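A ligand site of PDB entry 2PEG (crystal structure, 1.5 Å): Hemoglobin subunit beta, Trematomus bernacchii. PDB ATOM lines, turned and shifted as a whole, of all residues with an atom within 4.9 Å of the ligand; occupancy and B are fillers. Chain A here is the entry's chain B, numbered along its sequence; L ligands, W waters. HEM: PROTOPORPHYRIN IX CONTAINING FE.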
ATOM      1  N   THR A  38      -9.009   7.248  -2.822  1.00  0.00           N
ATOM      2  CA  THR A  38      -9.127   6.217  -1.778  1.00  0.00           C
ATOM      3  C   THR A  38     -10.108   5.118  -2.211  1.00  0.00           C
ATOM      4  O   THR A  38     -10.228   4.042  -1.585  1.00  0.00           O
ATOM      5  CB  THR A  38      -9.602   6.843  -0.385  1.00  0.00           C
ATOM      6  OG1 THR A  38     -10.880   7.536  -0.535  1.00  0.00           O
ATOM      7  CG2 THR A  38      -8.521   7.787   0.168  1.00  0.00           C
ATOM      8  N   HIS A  41      -9.326   1.188  -2.837  1.00  0.00           N
ATOM      9  CA  HIS A  41      -9.375   0.101  -1.868  1.00  0.00           C
ATOM     10  C   HIS A  41     -10.650  -0.634  -1.713  1.00  0.00           C
ATOM     11  O   HIS A  41     -10.655  -1.702  -1.125  1.00  0.00           O
ATOM     12  CB  HIS A  41      -8.988   0.634  -0.506  1.00  0.00           C
ATOM     13  CG  HIS A  41      -7.642   1.246  -0.502  1.00  0.00           C
ATOM     14  ND1 HIS A  41      -6.483   0.486  -0.526  1.00  0.00           N
ATOM     15  CD2 HIS A  41      -7.246   2.535  -0.600  1.00  0.00           C
ATOM     16  CE1 HIS A  41      -5.431   1.280  -0.635  1.00  0.00           C
ATOM     17  NE2 HIS A  41      -5.870   2.529  -0.680  1.00  0.00           N
ATOM     18  N   PHE A  42     -11.721  -0.038  -2.200  1.00  0.00           N
ATOM     19  CA  PHE A  42     -13.010  -0.661  -2.012  1.00  0.00           C
ATOM     20  C   PHE A  42     -13.663  -1.138  -3.259  1.00  0.00           C
ATOM     21  O   PHE A  42     -14.827  -1.522  -3.226  1.00  0.00           O
ATOM     22  CB  PHE A  42     -13.913   0.261  -1.200  1.00  0.00           C
ATOM     23  CG  PHE A  42     -13.345   0.593   0.140  1.00  0.00           C
ATOM     24  CD1 PHE A  42     -13.469  -0.299   1.207  1.00  0.00           C
ATOM     25  CD2 PHE A  42     -12.544   1.719   0.314  1.00  0.00           C
ATOM     26  CE1 PHE A  42     -12.780  -0.060   2.412  1.00  0.00           C
ATOM     27  CE2 PHE A  42     -11.857   1.949   1.515  1.00  0.00           C
ATOM     28  CZ  PHE A  42     -11.975   1.066   2.562  1.00  0.00           C
ATOM     29  N   HIS A  63     -16.824  -1.498   5.972  1.00  0.00           N
ATOM     30  CA  HIS A  63     -15.529  -1.047   6.501  1.00  0.00           C
ATOM     31  C   HIS A  63     -15.693   0.256   7.329  1.00  0.00           C
ATOM     32  O   HIS A  63     -15.004   0.438   8.336  1.00  0.00           O
ATOM     33  CB  HIS A  63     -14.488  -0.874   5.366  1.00  0.00           C
ATOM     34  CG  HIS A  63     -13.216  -0.240   5.819  1.00  0.00           C
ATOM     35  ND1 HIS A  63     -12.965   1.113   5.748  1.00  0.00           N
ATOM     36  CD2 HIS A  63     -12.165  -0.781   6.473  1.00  0.00           C
ATOM     37  CE1 HIS A  63     -11.781   1.366   6.369  1.00  0.00           C
ATOM     38  NE2 HIS A  63     -11.252   0.259   6.830  1.00  0.00           N
ATOM     39  N   LYS A  66     -16.556  -0.819  10.645  1.00  0.00           N
ATOM     40  CA  LYS A  66     -15.351  -1.396  11.262  1.00  0.00           C
ATOM     41  C   LYS A  66     -14.443  -0.294  11.763  1.00  0.00           C
ATOM     42  O   LYS A  66     -13.838  -0.421  12.801  1.00  0.00           O
ATOM     43  CB  LYS A  66     -14.532  -2.207  10.252  1.00  0.00           C
ATOM     44  CG  LYS A  66     -15.098  -3.557   9.968  1.00  0.00           C
ATOM     45  CD  LYS A  66     -14.218  -4.265   9.002  1.00  0.00           C
ATOM     46  CE  LYS A  66     -14.961  -5.460   8.476  1.00  0.00           C
ATOM     47  NZ  LYS A  66     -14.021  -6.193   7.574  1.00  0.00           N
ATOM     48  N   VAL A  67     -14.285   0.770  10.990  1.00  0.00           N
ATOM     49  CA  VAL A  67     -13.436   1.870  11.433  1.00  0.00           C
ATOM     50  C   VAL A  67     -13.881   2.409  12.804  1.00  0.00           C
ATOM     51  O   VAL A  67     -13.061   2.603  13.688  1.00  0.00           O
ATOM     52  CB  VAL A  67     -13.469   3.023  10.418  1.00  0.00           C
ATOM     53  CG1 VAL A  67     -12.829   4.276  11.006  1.00  0.00           C
ATOM     54  CG2 VAL A  67     -12.724   2.580   9.155  1.00  0.00           C
ATOM     55  N   GLY A  70     -13.242   0.100  15.455  1.00  0.00           N
ATOM     56  CA  GLY A  70     -11.809   0.125  15.663  1.00  0.00           C
ATOM     57  C   GLY A  70     -11.340   1.268  16.576  1.00  0.00           C
ATOM     58  O   GLY A  70     -10.368   1.120  17.304  1.00  0.00           O
ATOM     59  N   LEU A  71     -12.015   2.408  16.529  1.00  0.00           N
ATOM     60  CA  LEU A  71     -11.669   3.585  17.341  1.00  0.00           C
ATOM     61  C   LEU A  71     -12.050   3.328  18.775  1.00  0.00           C
ATOM     62  O   LEU A  71     -11.429   3.845  19.698  1.00  0.00           O
ATOM     63  CB  LEU A  71     -12.401   4.830  16.835  1.00  0.00           C
ATOM     64  CG  LEU A  71     -11.965   5.248  15.445  1.00  0.00           C
ATOM     65  CD1 LEU A  71     -12.773   6.382  14.919  1.00  0.00           C
ATOM     66  CD2 LEU A  71     -10.536   5.600  15.536  1.00  0.00           C
ATOM     67  N   ARG A  73     -11.562   0.700  20.674  1.00  0.00           N
ATOM     68  CA  ARG A  73     -10.553   0.123  21.545  1.00  0.00           C
ATOM     69  C   ARG A  73      -9.587   1.211  21.962  1.00  0.00           C
ATOM     70  O   ARG A  73      -8.932   1.090  22.990  1.00  0.00           O
ATOM     71  CB  ARG A  73      -9.843  -1.003  20.830  1.00  0.00           C
ATOM     72  CG  ARG A  73      -8.917  -0.510  19.771  1.00  0.00           C
ATOM     73  CD  ARG A  73      -8.280  -1.694  19.066  1.00  0.00           C
ATOM     74  NE  ARG A  73      -9.159  -2.275  18.066  1.00  0.00           N
ATOM     75  CZ  ARG A  73      -8.740  -3.249  17.291  1.00  0.00           C
ATOM     76  NH1 ARG A  73      -7.516  -3.716  17.493  1.00  0.00           N
ATOM     77  NH2 ARG A  73      -9.480  -3.714  16.275  1.00  0.00           N
ATOM     78  N   TYR A  85      -2.890   0.100  18.224  1.00  0.00           N
ATOM     79  CA  TYR A  85      -3.053   0.084  16.772  1.00  0.00           C
ATOM     80  C   TYR A  85      -1.879  -0.467  15.952  1.00  0.00           C
ATOM     81  O   TYR A  85      -1.906  -0.429  14.733  1.00  0.00           O
ATOM     82  CB  TYR A  85      -3.405   1.489  16.284  1.00  0.00           C
ATOM     83  CG  TYR A  85      -4.782   1.854  16.776  1.00  0.00           C
ATOM     84  CD1 TYR A  85      -4.966   2.697  17.876  1.00  0.00           C
ATOM     85  CD2 TYR A  85      -5.916   1.327  16.172  1.00  0.00           C
ATOM     86  CE1 TYR A  85      -6.256   2.989  18.361  1.00  0.00           C
ATOM     87  CE2 TYR A  85      -7.200   1.615  16.642  1.00  0.00           C
ATOM     88  CZ  TYR A  85      -7.369   2.439  17.726  1.00  0.00           C
ATOM     89  OH  TYR A  85      -8.634   2.744  18.154  1.00  0.00           O
ATOM     90  N   LEU A  88      -3.018  -3.217  13.515  1.00  0.00           N
ATOM     91  CA  LEU A  88      -3.876  -2.703  12.461  1.00  0.00           C
ATOM     92  C   LEU A  88      -3.004  -1.851  11.530  1.00  0.00           C
ATOM     93  O   LEU A  88      -3.266  -1.762  10.356  1.00  0.00           O
ATOM     94  CB  LEU A  88      -5.011  -1.833  13.030  1.00  0.00           C
ATOM     95  CG  LEU A  88      -6.397  -2.455  13.280  1.00  0.00           C
ATOM     96  CD1 LEU A  88      -7.390  -1.312  13.710  1.00  0.00           C
ATOM     97  CD2 LEU A  88      -6.907  -3.166  12.001  1.00  0.00           C
ATOM     98  N   LEU A  91      -1.224  -4.196   9.121  1.00  0.00           N
ATOM     99  CA  LEU A  91      -2.195  -4.747   8.188  1.00  0.00           C
ATOM    100  C   LEU A  91      -2.418  -3.777   7.031  1.00  0.00           C
ATOM    101  O   LEU A  91      -2.232  -4.116   5.870  1.00  0.00           O
ATOM    102  CB  LEU A  91      -3.524  -4.980   8.899  1.00  0.00           C
ATOM    103  CG  LEU A  91      -4.633  -5.462   7.982  1.00  0.00           C
ATOM    104  CD1 LEU A  91      -4.285  -6.850   7.543  1.00  0.00           C
ATOM    105  CD2 LEU A  91      -5.973  -5.438   8.669  1.00  0.00           C
ATOM    106  N   HIS A  92      -2.839  -2.533   7.359  1.00  0.00           N
ATOM    107  CA  HIS A  92      -3.114  -1.520   6.336  1.00  0.00           C
ATOM    108  C   HIS A  92      -1.893  -1.170   5.449  1.00  0.00           C
ATOM    109  O   HIS A  92      -2.071  -0.961   4.251  1.00  0.00           O
ATOM    110  CB  HIS A  92      -3.708  -0.233   6.983  1.00  0.00           C
ATOM    111  CG  HIS A  92      -5.133  -0.397   7.428  1.00  0.00           C
ATOM    112  ND1 HIS A  92      -5.526  -1.070   8.563  1.00  0.00           N
ATOM    113  CD2 HIS A  92      -6.286   0.014   6.843  1.00  0.00           C
ATOM    114  CE1 HIS A  92      -6.870  -1.048   8.644  1.00  0.00           C
ATOM    115  NE2 HIS A  92      -7.396  -0.394   7.621  1.00  0.00           N
ATOM    116  N   LEU A  96      -2.498  -4.152   2.925  1.00  0.00           N
ATOM    117  CA  LEU A  96      -3.443  -3.421   2.128  1.00  0.00           C
ATOM    118  C   LEU A  96      -2.835  -2.297   1.272  1.00  0.00           C
ATOM    119  O   LEU A  96      -3.503  -1.802   0.370  1.00  0.00           O
ATOM    120  CB  LEU A  96      -4.555  -2.883   3.056  1.00  0.00           C
ATOM    121  CG  LEU A  96      -5.239  -3.970   3.895  1.00  0.00           C
ATOM    122  CD1 LEU A  96      -6.215  -3.345   4.908  1.00  0.00           C
ATOM    123  CD2 LEU A  96      -5.958  -4.923   2.944  1.00  0.00           C
ATOM    124  N   VAL A  98      -2.321   0.773   2.005  1.00  0.00           N
ATOM    125  CA  VAL A  98      -3.043   2.008   2.168  1.00  0.00           C
ATOM    126  C   VAL A  98      -1.972   3.064   2.385  1.00  0.00           C
ATOM    127  O   VAL A  98      -1.106   2.857   3.225  1.00  0.00           O
ATOM    128  CB  VAL A  98      -3.980   1.928   3.389  1.00  0.00           C
ATOM    129  CG1 VAL A  98      -4.580   3.315   3.716  1.00  0.00           C
ATOM    130  CG2 VAL A  98      -5.061   0.889   3.101  1.00  0.00           C
ATOM    131  N   ASN A 102      -3.739   8.760   3.828  1.00  0.00           N
ATOM    132  CA  ASN A 102      -5.172   8.495   3.812  1.00  0.00           C
ATOM    133  C   ASN A 102      -5.861   8.526   5.175  1.00  0.00           C
ATOM    134  O   ASN A 102      -7.032   8.837   5.248  1.00  0.00           O
ATOM    135  CB  ASN A 102      -5.484   7.143   3.187  1.00  0.00           C
ATOM    136  CG  ASN A 102      -5.121   7.062   1.725  1.00  0.00           C
ATOM    137  OD1 ASN A 102      -4.752   8.062   1.073  1.00  0.00           O
ATOM    138  ND2 ASN A 102      -5.243   5.855   1.182  1.00  0.00           N
ATOM    139  N   PHE A 103      -5.134   8.183   6.244  1.00  0.00           N
ATOM    140  CA  PHE A 103      -5.768   8.167   7.589  1.00  0.00           C
ATOM    141  C   PHE A 103      -6.177   9.568   8.029  1.00  0.00           C
ATOM    142  O   PHE A 103      -7.220   9.730   8.635  1.00  0.00           O
ATOM    143  CB  PHE A 103      -4.831   7.536   8.614  1.00  0.00           C
ATOM    144  CG  PHE A 103      -4.481   6.131   8.294  1.00  0.00           C
ATOM    145  CD1 PHE A 103      -5.473   5.133   8.328  1.00  0.00           C
ATOM    146  CD2 PHE A 103      -3.201   5.821   7.848  1.00  0.00           C
ATOM    147  CE1 PHE A 103      -5.188   3.817   7.911  1.00  0.00           C
ATOM    148  CE2 PHE A 103      -2.886   4.538   7.419  1.00  0.00           C
ATOM    149  CZ  PHE A 103      -3.892   3.524   7.446  1.00  0.00           C
ATOM    150  N   LEU A 106      -9.313  10.600   5.999  1.00  0.00           N
ATOM    151  CA  LEU A 106     -10.508   9.954   6.541  1.00  0.00           C
ATOM    152  C   LEU A 106     -10.903  10.562   7.891  1.00  0.00           C
ATOM    153  O   LEU A 106     -12.111  10.747   8.151  1.00  0.00           O
ATOM    154  CB  LEU A 106     -10.280   8.420   6.713  1.00  0.00           C
ATOM    155  CG  LEU A 106     -11.412   7.689   7.414  1.00  0.00           C
ATOM    156  CD1 LEU A 106     -12.768   7.927   6.675  1.00  0.00           C
ATOM    157  CD2 LEU A 106     -11.042   6.170   7.498  1.00  0.00           C
ATOM    158  N   VAL A 137      -4.595   8.464  16.980  1.00  0.00           N
ATOM    159  CA  VAL A 137      -4.870   7.197  16.288  1.00  0.00           C
ATOM    160  C   VAL A 137      -4.236   7.183  14.914  1.00  0.00           C
ATOM    161  O   VAL A 137      -3.624   6.179  14.511  1.00  0.00           O
ATOM    162  CB  VAL A 137      -6.422   6.935  16.186  1.00  0.00           C
ATOM    163  CG1 VAL A 137      -6.727   5.711  15.314  1.00  0.00           C
ATOM    164  CG2 VAL A 137      -6.982   6.721  17.610  1.00  0.00           C
ATOM    165  N   LEU A 141      -1.557   4.605  13.250  1.00  0.00           N
ATOM    166  CA  LEU A 141      -1.852   3.872  12.032  1.00  0.00           C
ATOM    167  C   LEU A 141      -0.848   4.183  10.916  1.00  0.00           C
ATOM    168  O   LEU A 141      -0.387   3.279  10.231  1.00  0.00           O
ATOM    169  CB  LEU A 141      -3.293   4.233  11.576  1.00  0.00           C
ATOM    170  CG  LEU A 141      -4.412   3.604  12.405  1.00  0.00           C
ATOM    171  CD1 LEU A 141      -5.759   4.107  11.924  1.00  0.00           C
ATOM    172  CD2 LEU A 141      -4.339   2.064  12.305  1.00  0.00           C
HETATM  173  CHA HEM L   1      -9.834  -3.474   7.030  1.00  0.00           C
HETATM  174  CHB HEM L   1     -10.029  -0.298  10.720  1.00  0.00           C
HETATM  175  CHC HEM L   1      -8.618   3.329   7.730  1.00  0.00           C
HETATM  176  CHD HEM L   1      -8.843   0.270   3.971  1.00  0.00           C
HETATM  177  C1A HEM L   1      -9.933  -2.904   8.328  1.00  0.00           C
HETATM  178  C2A HEM L   1     -10.390  -3.649   9.473  1.00  0.00           C
HETATM  179  C3A HEM L   1     -10.510  -2.719  10.488  1.00  0.00           C
HETATM  180  C4A HEM L   1     -10.111  -1.434   9.983  1.00  0.00           C
HETATM  181  CMA HEM L   1     -11.001  -2.987  11.945  1.00  0.00           C
HETATM  182  CAA HEM L   1     -10.630  -5.189   9.480  1.00  0.00           C
HETATM  183  CBA HEM L   1      -9.208  -5.536   9.830  1.00  0.00           C
HETATM  184  CGA HEM L   1      -8.973  -6.994  10.008  1.00  0.00           C
HETATM  185  O1A HEM L   1      -8.121  -7.398  10.879  1.00  0.00           O
HETATM  186  O2A HEM L   1      -9.619  -7.749   9.262  1.00  0.00           O
HETATM  187  C1B HEM L   1      -9.641   0.955  10.258  1.00  0.00           C
HETATM  188  C2B HEM L   1      -9.404   2.069  11.168  1.00  0.00           C
HETATM  189  C3B HEM L   1      -9.028   3.064  10.261  1.00  0.00           C
HETATM  190  C4B HEM L   1      -9.025   2.589   8.866  1.00  0.00           C
HETATM  191  CMB HEM L   1      -9.605   2.122  12.724  1.00  0.00           C
HETATM  192  CAB HEM L   1      -8.692   4.432  10.474  1.00  0.00           C
HETATM  193  CBB HEM L   1      -9.107   5.149  11.560  1.00  0.00           C
HETATM  194  C1C HEM L   1      -8.579   2.879   6.448  1.00  0.00           C
HETATM  195  C2C HEM L   1      -8.311   3.710   5.284  1.00  0.00           C
HETATM  196  C3C HEM L   1      -8.432   2.790   4.196  1.00  0.00           C
HETATM  197  C4C HEM L   1      -8.774   1.483   4.721  1.00  0.00           C
HETATM  198  CMC HEM L   1      -8.215   5.275   5.246  1.00  0.00           C
HETATM  199  CAC HEM L   1      -8.339   2.999   2.820  1.00  0.00           C
HETATM  200  CBC HEM L   1      -8.558   4.209   2.255  1.00  0.00           C
HETATM  201  C1D HEM L   1      -9.053  -1.051   4.489  1.00  0.00           C
HETATM  202  C2D HEM L   1      -9.362  -2.267   3.669  1.00  0.00           C
HETATM  203  C3D HEM L   1      -9.643  -3.267   4.548  1.00  0.00           C
HETATM  204  C4D HEM L   1      -9.515  -2.755   5.883  1.00  0.00           C
HETATM  205  CMD HEM L   1      -9.228  -2.375   2.181  1.00  0.00           C
HETATM  206  CAD HEM L   1      -9.985  -4.674   4.148  1.00  0.00           C
HETATM  207  CBD HEM L   1     -11.456  -4.659   3.771  1.00  0.00           C
HETATM  208  CGD HEM L   1     -12.371  -4.683   4.983  1.00  0.00           C
HETATM  209  O1D HEM L   1     -12.044  -5.424   5.948  1.00  0.00           O
HETATM  210  O2D HEM L   1     -13.407  -3.986   5.009  1.00  0.00           O
HETATM  211  NA  HEM L   1      -9.790  -1.548   8.667  1.00  0.00           N
HETATM  212  NB  HEM L   1      -9.388   1.255   8.906  1.00  0.00           N
HETATM  213  NC  HEM L   1      -8.864   1.543   6.086  1.00  0.00           N
HETATM  214  ND  HEM L   1      -9.199  -1.341   5.842  1.00  0.00           N
HETATM  215 FE   HEM L   1      -9.319  -0.018   7.336  1.00  0.00          FE
HETATM  216  O   HOH W   1     -15.409  -3.700   3.291  1.00  0.00           O
HETATM  217  O   HOH W   2     -13.531  -2.904  14.238  1.00  0.00           O
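The backbone carbonyl oxygen of His 92 lies within hydrogen-bond range of the backbone NH of Val 98, at 2.8 Å. A ring nitrogen (ND1) of His 92 lies within hydrogen-bond range of the backbone carbonyl oxygen (O) of Leu 88 (3.0 Å). The backbone carbonyl oxygen of Leu 91 sits at hydrogen-bond distance from the backbone NH of Leu 96, 3.0 Å away.
The side-chain amino group (NZ) of Lys 66 is in salt-bridge range of an oxygen (O1D) of the ligand (2.7 Å). A ring nitrogen (NE2) of His 63 is bound to an iron atom (FE) of the ligand (2.0 Å). An iron atom (FE) of the ligand is bound by a ring nitrogen (NE2) of His 92.
Thr 38 touches the ligand. His 41 touches the ligand. Phe 42 touches the ligand (CZ to CHD, 3.5 Å). Val 67 touches the ligand. Leu 88 touches the ligand. CD2 of Leu 91 touches CBA of the ligand (3.4 Å). Leu 96 touches the ligand (CD1 to C3D, 3.4 Å). Val 98 touches the ligand (CG1 to CAC, 3.9 Å). Asn 102 touches the ligand. CE1 of Phe 103 touches CHC of the ligand (3.5 Å). CD2 of Leu 106 touches CMC of the ligand, 3.7 Å away. Leu 141 touches the ligand. Hydrophobic or aromatic side chains within 4 Å of the ligand: His 41, Phe 42, His 63, Val 67, Leu 88, Leu 91, His 92, Leu 96, Val 98, Phe 103, Leu 106 and Leu 141. Along chain A the residues within 4 Å of the ligand span positions 38 to 141.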
